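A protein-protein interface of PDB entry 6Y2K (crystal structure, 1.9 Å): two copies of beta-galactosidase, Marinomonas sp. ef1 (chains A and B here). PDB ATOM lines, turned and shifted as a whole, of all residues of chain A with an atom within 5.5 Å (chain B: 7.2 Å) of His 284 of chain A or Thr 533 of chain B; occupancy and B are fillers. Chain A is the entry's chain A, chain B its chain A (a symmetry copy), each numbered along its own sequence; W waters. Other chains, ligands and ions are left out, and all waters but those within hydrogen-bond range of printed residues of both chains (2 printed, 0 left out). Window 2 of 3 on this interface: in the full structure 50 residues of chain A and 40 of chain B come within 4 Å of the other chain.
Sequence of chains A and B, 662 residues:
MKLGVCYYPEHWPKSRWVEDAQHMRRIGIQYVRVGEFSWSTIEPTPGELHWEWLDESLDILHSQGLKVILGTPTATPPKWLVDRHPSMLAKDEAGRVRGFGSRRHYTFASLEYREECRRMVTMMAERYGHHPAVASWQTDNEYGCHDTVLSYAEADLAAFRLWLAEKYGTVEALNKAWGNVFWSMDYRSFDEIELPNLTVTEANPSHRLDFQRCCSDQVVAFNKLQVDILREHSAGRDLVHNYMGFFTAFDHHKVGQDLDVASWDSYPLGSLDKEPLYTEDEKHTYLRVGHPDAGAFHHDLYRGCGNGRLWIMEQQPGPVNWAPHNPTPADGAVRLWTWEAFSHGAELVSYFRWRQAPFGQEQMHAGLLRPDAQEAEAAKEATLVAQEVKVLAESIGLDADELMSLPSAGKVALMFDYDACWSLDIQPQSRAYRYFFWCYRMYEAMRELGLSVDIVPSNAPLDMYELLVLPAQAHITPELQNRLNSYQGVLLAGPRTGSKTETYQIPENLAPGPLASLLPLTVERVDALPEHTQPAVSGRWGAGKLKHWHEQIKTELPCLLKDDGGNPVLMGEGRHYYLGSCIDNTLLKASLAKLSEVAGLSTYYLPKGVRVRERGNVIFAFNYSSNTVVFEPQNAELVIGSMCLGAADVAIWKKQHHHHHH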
ATOM      1  N   THR A 279     -22.431  26.867  21.836  1.00  0.00           N
ATOM      2  CA  THR A 279     -21.700  26.782  20.580  1.00  0.00           C
ATOM      3  C   THR A 279     -21.987  25.472  19.867  1.00  0.00           C
ATOM      4  O   THR A 279     -22.505  24.513  20.456  1.00  0.00           O
ATOM      5  CB  THR A 279     -20.181  26.860  20.792  1.00  0.00           C
ATOM      6  OG1 THR A 279     -19.744  25.749  21.590  1.00  0.00           O
ATOM      7  CG2 THR A 279     -19.786  28.184  21.450  1.00  0.00           C
ATOM      8  N   GLU A 280     -21.610  25.427  18.593  1.00  0.00           N
ATOM      9  CA  GLU A 280     -21.741  24.189  17.817  1.00  0.00           C
ATOM     10  C   GLU A 280     -20.928  23.052  18.446  1.00  0.00           C
ATOM     11  O   GLU A 280     -21.436  21.930  18.570  1.00  0.00           O
ATOM     12  CB  GLU A 280     -21.385  24.393  16.334  1.00  0.00           C
ATOM     13  CG  GLU A 280     -22.611  24.671  15.469  1.00  0.00           C
ATOM     14  CD  GLU A 280     -23.608  25.589  16.156  1.00  0.00           C
ATOM     15  OE1 GLU A 280     -24.823  25.305  16.174  1.00  0.00           O
ATOM     16  OE2 GLU A 280     -23.155  26.608  16.709  1.00  0.00           O
ATOM     17  N   ASP A 281     -19.696  23.343  18.871  1.00  0.00           N
ATOM     18  CA  ASP A 281     -18.860  22.349  19.558  1.00  0.00           C
ATOM     19  C   ASP A 281     -19.517  21.802  20.830  1.00  0.00           C
ATOM     20  O   ASP A 281     -19.521  20.589  21.043  1.00  0.00           O
ATOM     21  CB  ASP A 281     -17.472  22.913  19.900  1.00  0.00           C
ATOM     22  CG  ASP A 281     -16.573  23.069  18.674  1.00  0.00           C
ATOM     23  OD1 ASP A 281     -16.891  22.526  17.585  1.00  0.00           O
ATOM     24  OD2 ASP A 281     -15.535  23.753  18.802  1.00  0.00           O
ATOM     25  N   GLU A 282     -20.078  22.683  21.653  1.00  0.00           N
ATOM     26  CA  GLU A 282     -20.799  22.261  22.873  1.00  0.00           C
ATOM     27  C   GLU A 282     -22.014  21.368  22.586  1.00  0.00           C
ATOM     28  O   GLU A 282     -22.232  20.355  23.274  1.00  0.00           O
ATOM     29  CB  GLU A 282     -21.231  23.474  23.695  1.00  0.00           C
ATOM     30  CG  GLU A 282     -20.059  24.180  24.377  1.00  0.00           C
ATOM     31  CD  GLU A 282     -20.420  25.521  25.008  1.00  0.00           C
ATOM     32  OE1 GLU A 282     -21.343  26.216  24.537  1.00  0.00           O
ATOM     33  OE2 GLU A 282     -19.745  25.912  25.974  1.00  0.00           O
ATOM     34  N   LYS A 283     -22.796  21.745  21.579  1.00  0.00           N
ATOM     35  CA  LYS A 283     -23.978  20.970  21.180  1.00  0.00           C
ATOM     36  C   LYS A 283     -23.604  19.562  20.741  1.00  0.00           C
ATOM     37  O   LYS A 283     -24.350  18.615  21.013  1.00  0.00           O
ATOM     38  CB  LYS A 283     -24.759  21.678  20.061  1.00  0.00           C
ATOM     39  CG  LYS A 283     -25.454  22.951  20.528  1.00  0.00           C
ATOM     40  CD  LYS A 283     -26.040  23.746  19.366  1.00  0.00           C
ATOM     41  CE  LYS A 283     -26.586  25.092  19.818  1.00  0.00           C
ATOM     42  NZ  LYS A 283     -27.862  24.977  20.581  1.00  0.00           N
ATOM     43  N   HIS A 284     -22.451  19.432  20.080  1.00  0.00           N
ATOM     44  CA  HIS A 284     -21.938  18.141  19.636  1.00  0.00           C
ATOM     45  C   HIS A 284     -21.300  17.362  20.790  1.00  0.00           C
ATOM     46  O   HIS A 284     -21.649  16.207  21.027  1.00  0.00           O
ATOM     47  CB  HIS A 284     -20.947  18.310  18.478  1.00  0.00           C
ATOM     48  CG  HIS A 284     -20.526  17.009  17.872  1.00  0.00           C
ATOM     49  ND1 HIS A 284     -19.326  16.404  18.176  1.00  0.00           N
ATOM     50  CD2 HIS A 284     -21.167  16.170  17.025  1.00  0.00           C
ATOM     51  CE1 HIS A 284     -19.238  15.255  17.528  1.00  0.00           C
ATOM     52  NE2 HIS A 284     -20.338  15.092  16.817  1.00  0.00           N
ATOM     53  N   THR A 285     -20.381  17.996  21.510  1.00  0.00           N
ATOM     54  CA  THR A 285     -19.643  17.338  22.604  1.00  0.00           C
ATOM     55  C   THR A 285     -20.544  16.796  23.697  1.00  0.00           C
ATOM     56  O   THR A 285     -20.339  15.687  24.181  1.00  0.00           O
ATOM     57  CB  THR A 285     -18.625  18.324  23.228  1.00  0.00           C
ATOM     58  OG1 THR A 285     -17.665  18.678  22.232  1.00  0.00           O
ATOM     59  CG2 THR A 285     -17.901  17.740  24.463  1.00  0.00           C
ATOM     60  N   TYR A 286     -21.547  17.578  24.082  1.00  0.00           N
ATOM     61  CA  TYR A 286     -22.382  17.254  25.238  1.00  0.00           C
ATOM     62  C   TYR A 286     -23.811  16.793  24.865  1.00  0.00           C
ATOM     63  O   TYR A 286     -24.707  16.778  25.723  1.00  0.00           O
ATOM     64  CB  TYR A 286     -22.417  18.477  26.155  1.00  0.00           C
ATOM     65  CG  TYR A 286     -21.069  18.849  26.743  1.00  0.00           C
ATOM     66  CD1 TYR A 286     -20.415  17.991  27.632  1.00  0.00           C
ATOM     67  CD2 TYR A 286     -20.446  20.062  26.419  1.00  0.00           C
ATOM     68  CE1 TYR A 286     -19.182  18.323  28.183  1.00  0.00           C
ATOM     69  CE2 TYR A 286     -19.215  20.406  26.972  1.00  0.00           C
ATOM     70  CZ  TYR A 286     -18.588  19.533  27.854  1.00  0.00           C
ATOM     71  OH  TYR A 286     -17.372  19.862  28.409  1.00  0.00           O
ATOM     72  N   LEU A 287     -24.011  16.400  23.600  1.00  0.00           N
ATOM     73  CA  LEU A 287     -25.315  15.969  23.072  1.00  0.00           C
ATOM     74  C   LEU A 287     -26.178  15.176  24.057  1.00  0.00           C
ATOM     75  O   LEU A 287     -27.359  15.452  24.187  1.00  0.00           O
ATOM     76  CB  LEU A 287     -25.109  15.088  21.828  1.00  0.00           C
ATOM     77  CG  LEU A 287     -26.348  14.509  21.140  1.00  0.00           C
ATOM     78  CD1 LEU A 287     -27.160  15.614  20.489  1.00  0.00           C
ATOM     79  CD2 LEU A 287     -25.952  13.473  20.105  1.00  0.00           C
ATOM     80  N   ARG A 288     -25.581  14.184  24.718  1.00  0.00           N
ATOM     81  CA  ARG A 288     -26.325  13.214  25.527  1.00  0.00           C
ATOM     82  C   ARG A 288     -26.288  13.450  27.039  1.00  0.00           C
ATOM     83  O   ARG A 288     -26.872  12.648  27.792  1.00  0.00           O
ATOM     84  CB  ARG A 288     -25.843  11.796  25.208  1.00  0.00           C
ATOM     85  CG  ARG A 288     -25.961  11.418  23.736  1.00  0.00           C
ATOM     86  CD  ARG A 288     -25.827   9.912  23.543  1.00  0.00           C
ATOM     87  NE  ARG A 288     -25.859   9.539  22.135  1.00  0.00           N
ATOM     88  CZ  ARG A 288     -26.956   9.484  21.376  1.00  0.00           C
ATOM     89  NH1 ARG A 288     -28.151   9.781  21.880  1.00  0.00           N
ATOM     90  NH2 ARG A 288     -26.852   9.135  20.096  1.00  0.00           N
ATOM     91  N   ASP B 527     -34.119   7.689  19.526  1.00  0.00           N
ATOM     92  CA  ASP B 527     -33.013   8.637  19.576  1.00  0.00           C
ATOM     93  C   ASP B 527     -33.160   9.512  18.315  1.00  0.00           C
ATOM     94  O   ASP B 527     -32.876   9.054  17.197  1.00  0.00           O
ATOM     95  CB  ASP B 527     -31.695   7.839  19.604  1.00  0.00           C
ATOM     96  CG  ASP B 527     -30.444   8.703  19.645  1.00  0.00           C
ATOM     97  OD1 ASP B 527     -30.464   9.799  20.228  1.00  0.00           O
ATOM     98  OD2 ASP B 527     -29.400   8.262  19.115  1.00  0.00           O
ATOM     99  N   LEU B 529     -32.137  12.640  16.147  1.00  0.00           N
ATOM    100  CA  LEU B 529     -30.785  13.202  16.049  1.00  0.00           C
ATOM    101  C   LEU B 529     -30.628  14.435  15.152  1.00  0.00           C
ATOM    102  O   LEU B 529     -31.292  14.548  14.112  1.00  0.00           O
ATOM    103  CB  LEU B 529     -29.822  12.114  15.551  1.00  0.00           C
ATOM    104  CG  LEU B 529     -29.519  10.962  16.511  1.00  0.00           C
ATOM    105  CD1 LEU B 529     -28.808   9.833  15.775  1.00  0.00           C
ATOM    106  CD2 LEU B 529     -28.703  11.419  17.715  1.00  0.00           C
ATOM    107  N   PRO B 530     -29.704  15.350  15.534  1.00  0.00           N
ATOM    108  CA  PRO B 530     -29.317  16.423  14.640  1.00  0.00           C
ATOM    109  C   PRO B 530     -28.350  15.894  13.583  1.00  0.00           C
ATOM    110  O   PRO B 530     -27.794  14.789  13.732  1.00  0.00           O
ATOM    111  CB  PRO B 530     -28.614  17.412  15.573  1.00  0.00           C
ATOM    112  CG  PRO B 530     -27.986  16.545  16.618  1.00  0.00           C
ATOM    113  CD  PRO B 530     -28.912  15.371  16.785  1.00  0.00           C
ATOM    114  N   GLU B 531     -28.129  16.697  12.544  1.00  0.00           N
ATOM    115  CA  GLU B 531     -27.247  16.328  11.425  1.00  0.00           C
ATOM    116  C   GLU B 531     -25.807  16.025  11.868  1.00  0.00           C
ATOM    117  O   GLU B 531     -25.133  15.171  11.275  1.00  0.00           O
ATOM    118  CB  GLU B 531     -27.251  17.455  10.376  1.00  0.00           C
ATOM    119  CG  GLU B 531     -26.554  17.134   9.054  1.00  0.00           C
ATOM    120  CD  GLU B 531     -27.285  16.103   8.200  1.00  0.00           C
ATOM    121  OE1 GLU B 531     -28.502  15.905   8.346  1.00  0.00           O
ATOM    122  OE2 GLU B 531     -26.627  15.486   7.352  1.00  0.00           O
ATOM    123  N   HIS B 532     -25.350  16.695  12.924  1.00  0.00           N
ATOM    124  CA  HIS B 532     -23.959  16.580  13.385  1.00  0.00           C
ATOM    125  C   HIS B 532     -23.544  15.281  14.085  1.00  0.00           C
ATOM    126  O   HIS B 532     -22.354  15.065  14.306  1.00  0.00           O
ATOM    127  CB  HIS B 532     -23.557  17.796  14.250  1.00  0.00           C
ATOM    128  CG  HIS B 532     -24.322  17.945  15.540  1.00  0.00           C
ATOM    129  ND1 HIS B 532     -24.138  17.111  16.623  1.00  0.00           N
ATOM    130  CD2 HIS B 532     -25.222  18.883  15.936  1.00  0.00           C
ATOM    131  CE1 HIS B 532     -24.916  17.509  17.618  1.00  0.00           C
ATOM    132  NE2 HIS B 532     -25.578  18.588  17.230  1.00  0.00           N
ATOM    133  N   THR B 533     -24.505  14.423  14.428  1.00  0.00           N
ATOM    134  CA  THR B 533     -24.225  13.156  15.097  1.00  0.00           C
ATOM    135  C   THR B 533     -24.854  12.010  14.300  1.00  0.00           C
ATOM    136  O   THR B 533     -26.072  11.861  14.270  1.00  0.00           O
ATOM    137  CB  THR B 533     -24.701  13.181  16.568  1.00  0.00           C
ATOM    138  OG1 THR B 533     -24.030  14.248  17.251  1.00  0.00           O
ATOM    139  CG2 THR B 533     -24.396  11.867  17.287  1.00  0.00           C
ATOM    140  N   GLN B 534     -23.994  11.218  13.658  1.00  0.00           N
ATOM    141  CA  GLN B 534     -24.366  10.156  12.734  1.00  0.00           C
ATOM    142  C   GLN B 534     -23.682   8.845  13.155  1.00  0.00           C
ATOM    143  O   GLN B 534     -22.562   8.551  12.721  1.00  0.00           O
ATOM    144  CB  GLN B 534     -23.980  10.567  11.311  1.00  0.00           C
ATOM    145  CG  GLN B 534     -24.733  11.803  10.846  1.00  0.00           C
ATOM    146  CD  GLN B 534     -24.529  12.158   9.378  1.00  0.00           C
ATOM    147  OE1 GLN B 534     -24.004  11.365   8.589  1.00  0.00           O
ATOM    148  NE2 GLN B 534     -24.953  13.370   9.005  1.00  0.00           N
ATOM    149  N   PRO B 535     -24.337   8.065  14.039  1.00  0.00           N
ATOM    150  CA  PRO B 535     -23.750   6.823  14.564  1.00  0.00           C
ATOM    151  C   PRO B 535     -23.301   5.806  13.505  1.00  0.00           C
ATOM    152  O   PRO B 535     -23.945   5.678  12.445  1.00  0.00           O
ATOM    153  CB  PRO B 535     -24.887   6.240  15.411  1.00  0.00           C
ATOM    154  CG  PRO B 535     -25.649   7.431  15.874  1.00  0.00           C
ATOM    155  CD  PRO B 535     -25.612   8.383  14.711  1.00  0.00           C
ATOM    156  N   LEU B 546     -25.775   5.982  10.121  1.00  0.00           N
ATOM    157  CA  LEU B 546     -27.182   6.347  10.197  1.00  0.00           C
ATOM    158  C   LEU B 546     -27.285   7.802  10.637  1.00  0.00           C
ATOM    159  O   LEU B 546     -26.378   8.324  11.282  1.00  0.00           O
ATOM    160  CB  LEU B 546     -27.917   5.436  11.174  1.00  0.00           C
ATOM    161  CG  LEU B 546     -27.624   5.575  12.675  1.00  0.00           C
ATOM    162  CD1 LEU B 546     -28.551   6.586  13.350  1.00  0.00           C
ATOM    163  CD2 LEU B 546     -27.767   4.216  13.334  1.00  0.00           C
ATOM    164  N   LYS B 547     -28.399   8.445  10.294  1.00  0.00           N
ATOM    165  CA  LYS B 547     -28.652   9.835  10.655  1.00  0.00           C
ATOM    166  C   LYS B 547     -30.123  10.073  10.967  1.00  0.00           C
ATOM    167  O   LYS B 547     -30.985   9.307  10.537  1.00  0.00           O
ATOM    168  CB  LYS B 547     -28.199  10.776   9.535  1.00  0.00           C
ATOM    169  CG  LYS B 547     -28.779  10.477   8.163  1.00  0.00           C
ATOM    170  CD  LYS B 547     -28.045  11.273   7.085  1.00  0.00           C
ATOM    171  CE  LYS B 547     -28.611  11.000   5.693  1.00  0.00           C
ATOM    172  NZ  LYS B 547     -28.034  11.941   4.680  1.00  0.00           N
ATOM    173  N   HIS B 548     -30.385  11.110  11.759  1.00  0.00           N
ATOM    174  CA  HIS B 548     -31.726  11.692  11.989  1.00  0.00           C
ATOM    175  C   HIS B 548     -32.650  10.925  12.923  1.00  0.00           C
ATOM    176  O   HIS B 548     -33.286  11.532  13.803  1.00  0.00           O
ATOM    177  CB  HIS B 548     -32.480  11.979  10.670  1.00  0.00           C
ATOM    178  CG  HIS B 548     -31.690  12.776   9.677  1.00  0.00           C
ATOM    179  ND1 HIS B 548     -31.899  12.680   8.317  1.00  0.00           N
ATOM    180  CD2 HIS B 548     -30.699  13.685   9.845  1.00  0.00           C
ATOM    181  CE1 HIS B 548     -31.065  13.491   7.690  1.00  0.00           C
ATOM    182  NE2 HIS B 548     -30.328  14.114   8.594  1.00  0.00           N
HETATM  183  O   HOH W   1     -20.138  16.357  13.711  1.00  0.00           O
HETATM  184  O   HOH W   2     -22.324  13.947  19.496  1.00  0.00           O
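Water W1 lies within hydrogen-bond range of the backbone carbonyl oxygen of His 532 of chain B (2.6 Å) and a ring nitrogen (NE2) of His 284 of chain A (3.4 Å). Water W2 bridges the backbone carbonyl oxygen (O) of His 284 of chain A and the side-chain hydroxyl (OG1) of Thr 533 of chain B.
Lys 283 of chain A touches His 532 of chain B. CD2 of His 284 of chain A touches OG1 of Thr 533 of chain B (3.5 Å). Leu 287 of chain A touches Thr 533 of chain B. CD2 of Leu 529 of chain B touches NH2 of Arg 288 of chain A (3.8 Å).
The guanidinium group of Arg 288 of chain A is in salt-bridge range of the side-chain carboxylate of Asp 527 of chain B (2.8 Å). O of His 532 of chain B lies close to NE2 of His 284 of chain A, at 3.2 Å.
Of the 11 printed residues of chain B, 4 touch a printed residue of chain A. Hydrophobic or aromatic side chains of chain B that line the printed part of chain A: Leu 529 and His 532. Among the printed residues, 6 pairs touch across the chains. Among the printed residues, Asp or Glu carboxylates within 4 Å of a Lys or Arg side-chain nitrogen of the other chain: Arg 288 of chain A with Asp 527 of chain B (2.8 Å).
No position is printed for both chains. Of the 6 pairs that touch across the chains among the printed residues, none has its exchanged pair printed and touching as well.
ND1 of His 532 of chain B is in hydrogen-bond range of OG1 of Thr 533 of chain B (2.9 Å). The backbone NH (N) of Leu 529 of chain B lies within hydrogen-bond range of the backbone carbonyl oxygen (O) of His 548 of chain B, 2.8 Å away.
Of chain B, only His 532 (3.1 Å) and Thr 533 (3.5 Å) come within 4 Å of His 284 of chain A. Of chain A, only His 284 (3.5 Å) and Leu 287 (3.5 Å) come within 4 Å of Thr 533 of chain B. Of the printed residues of chain B, Leu 287 of chain A touches Thr 533 (3.5 Å). Of the printed residues of chain B, Arg 288 of chain A touches Asp 527 (2.8 Å) and Leu 529 (3.8 Å). Of the printed residues of chain A, Leu 529 of chain B touches Arg 288. Printed residues of chain A within 4 Å of Asp 527 of chain B: Arg 288 (2.8 Å). Of the printed residues of chain A, His 532 of chain B touches Lys 283 and His 284.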
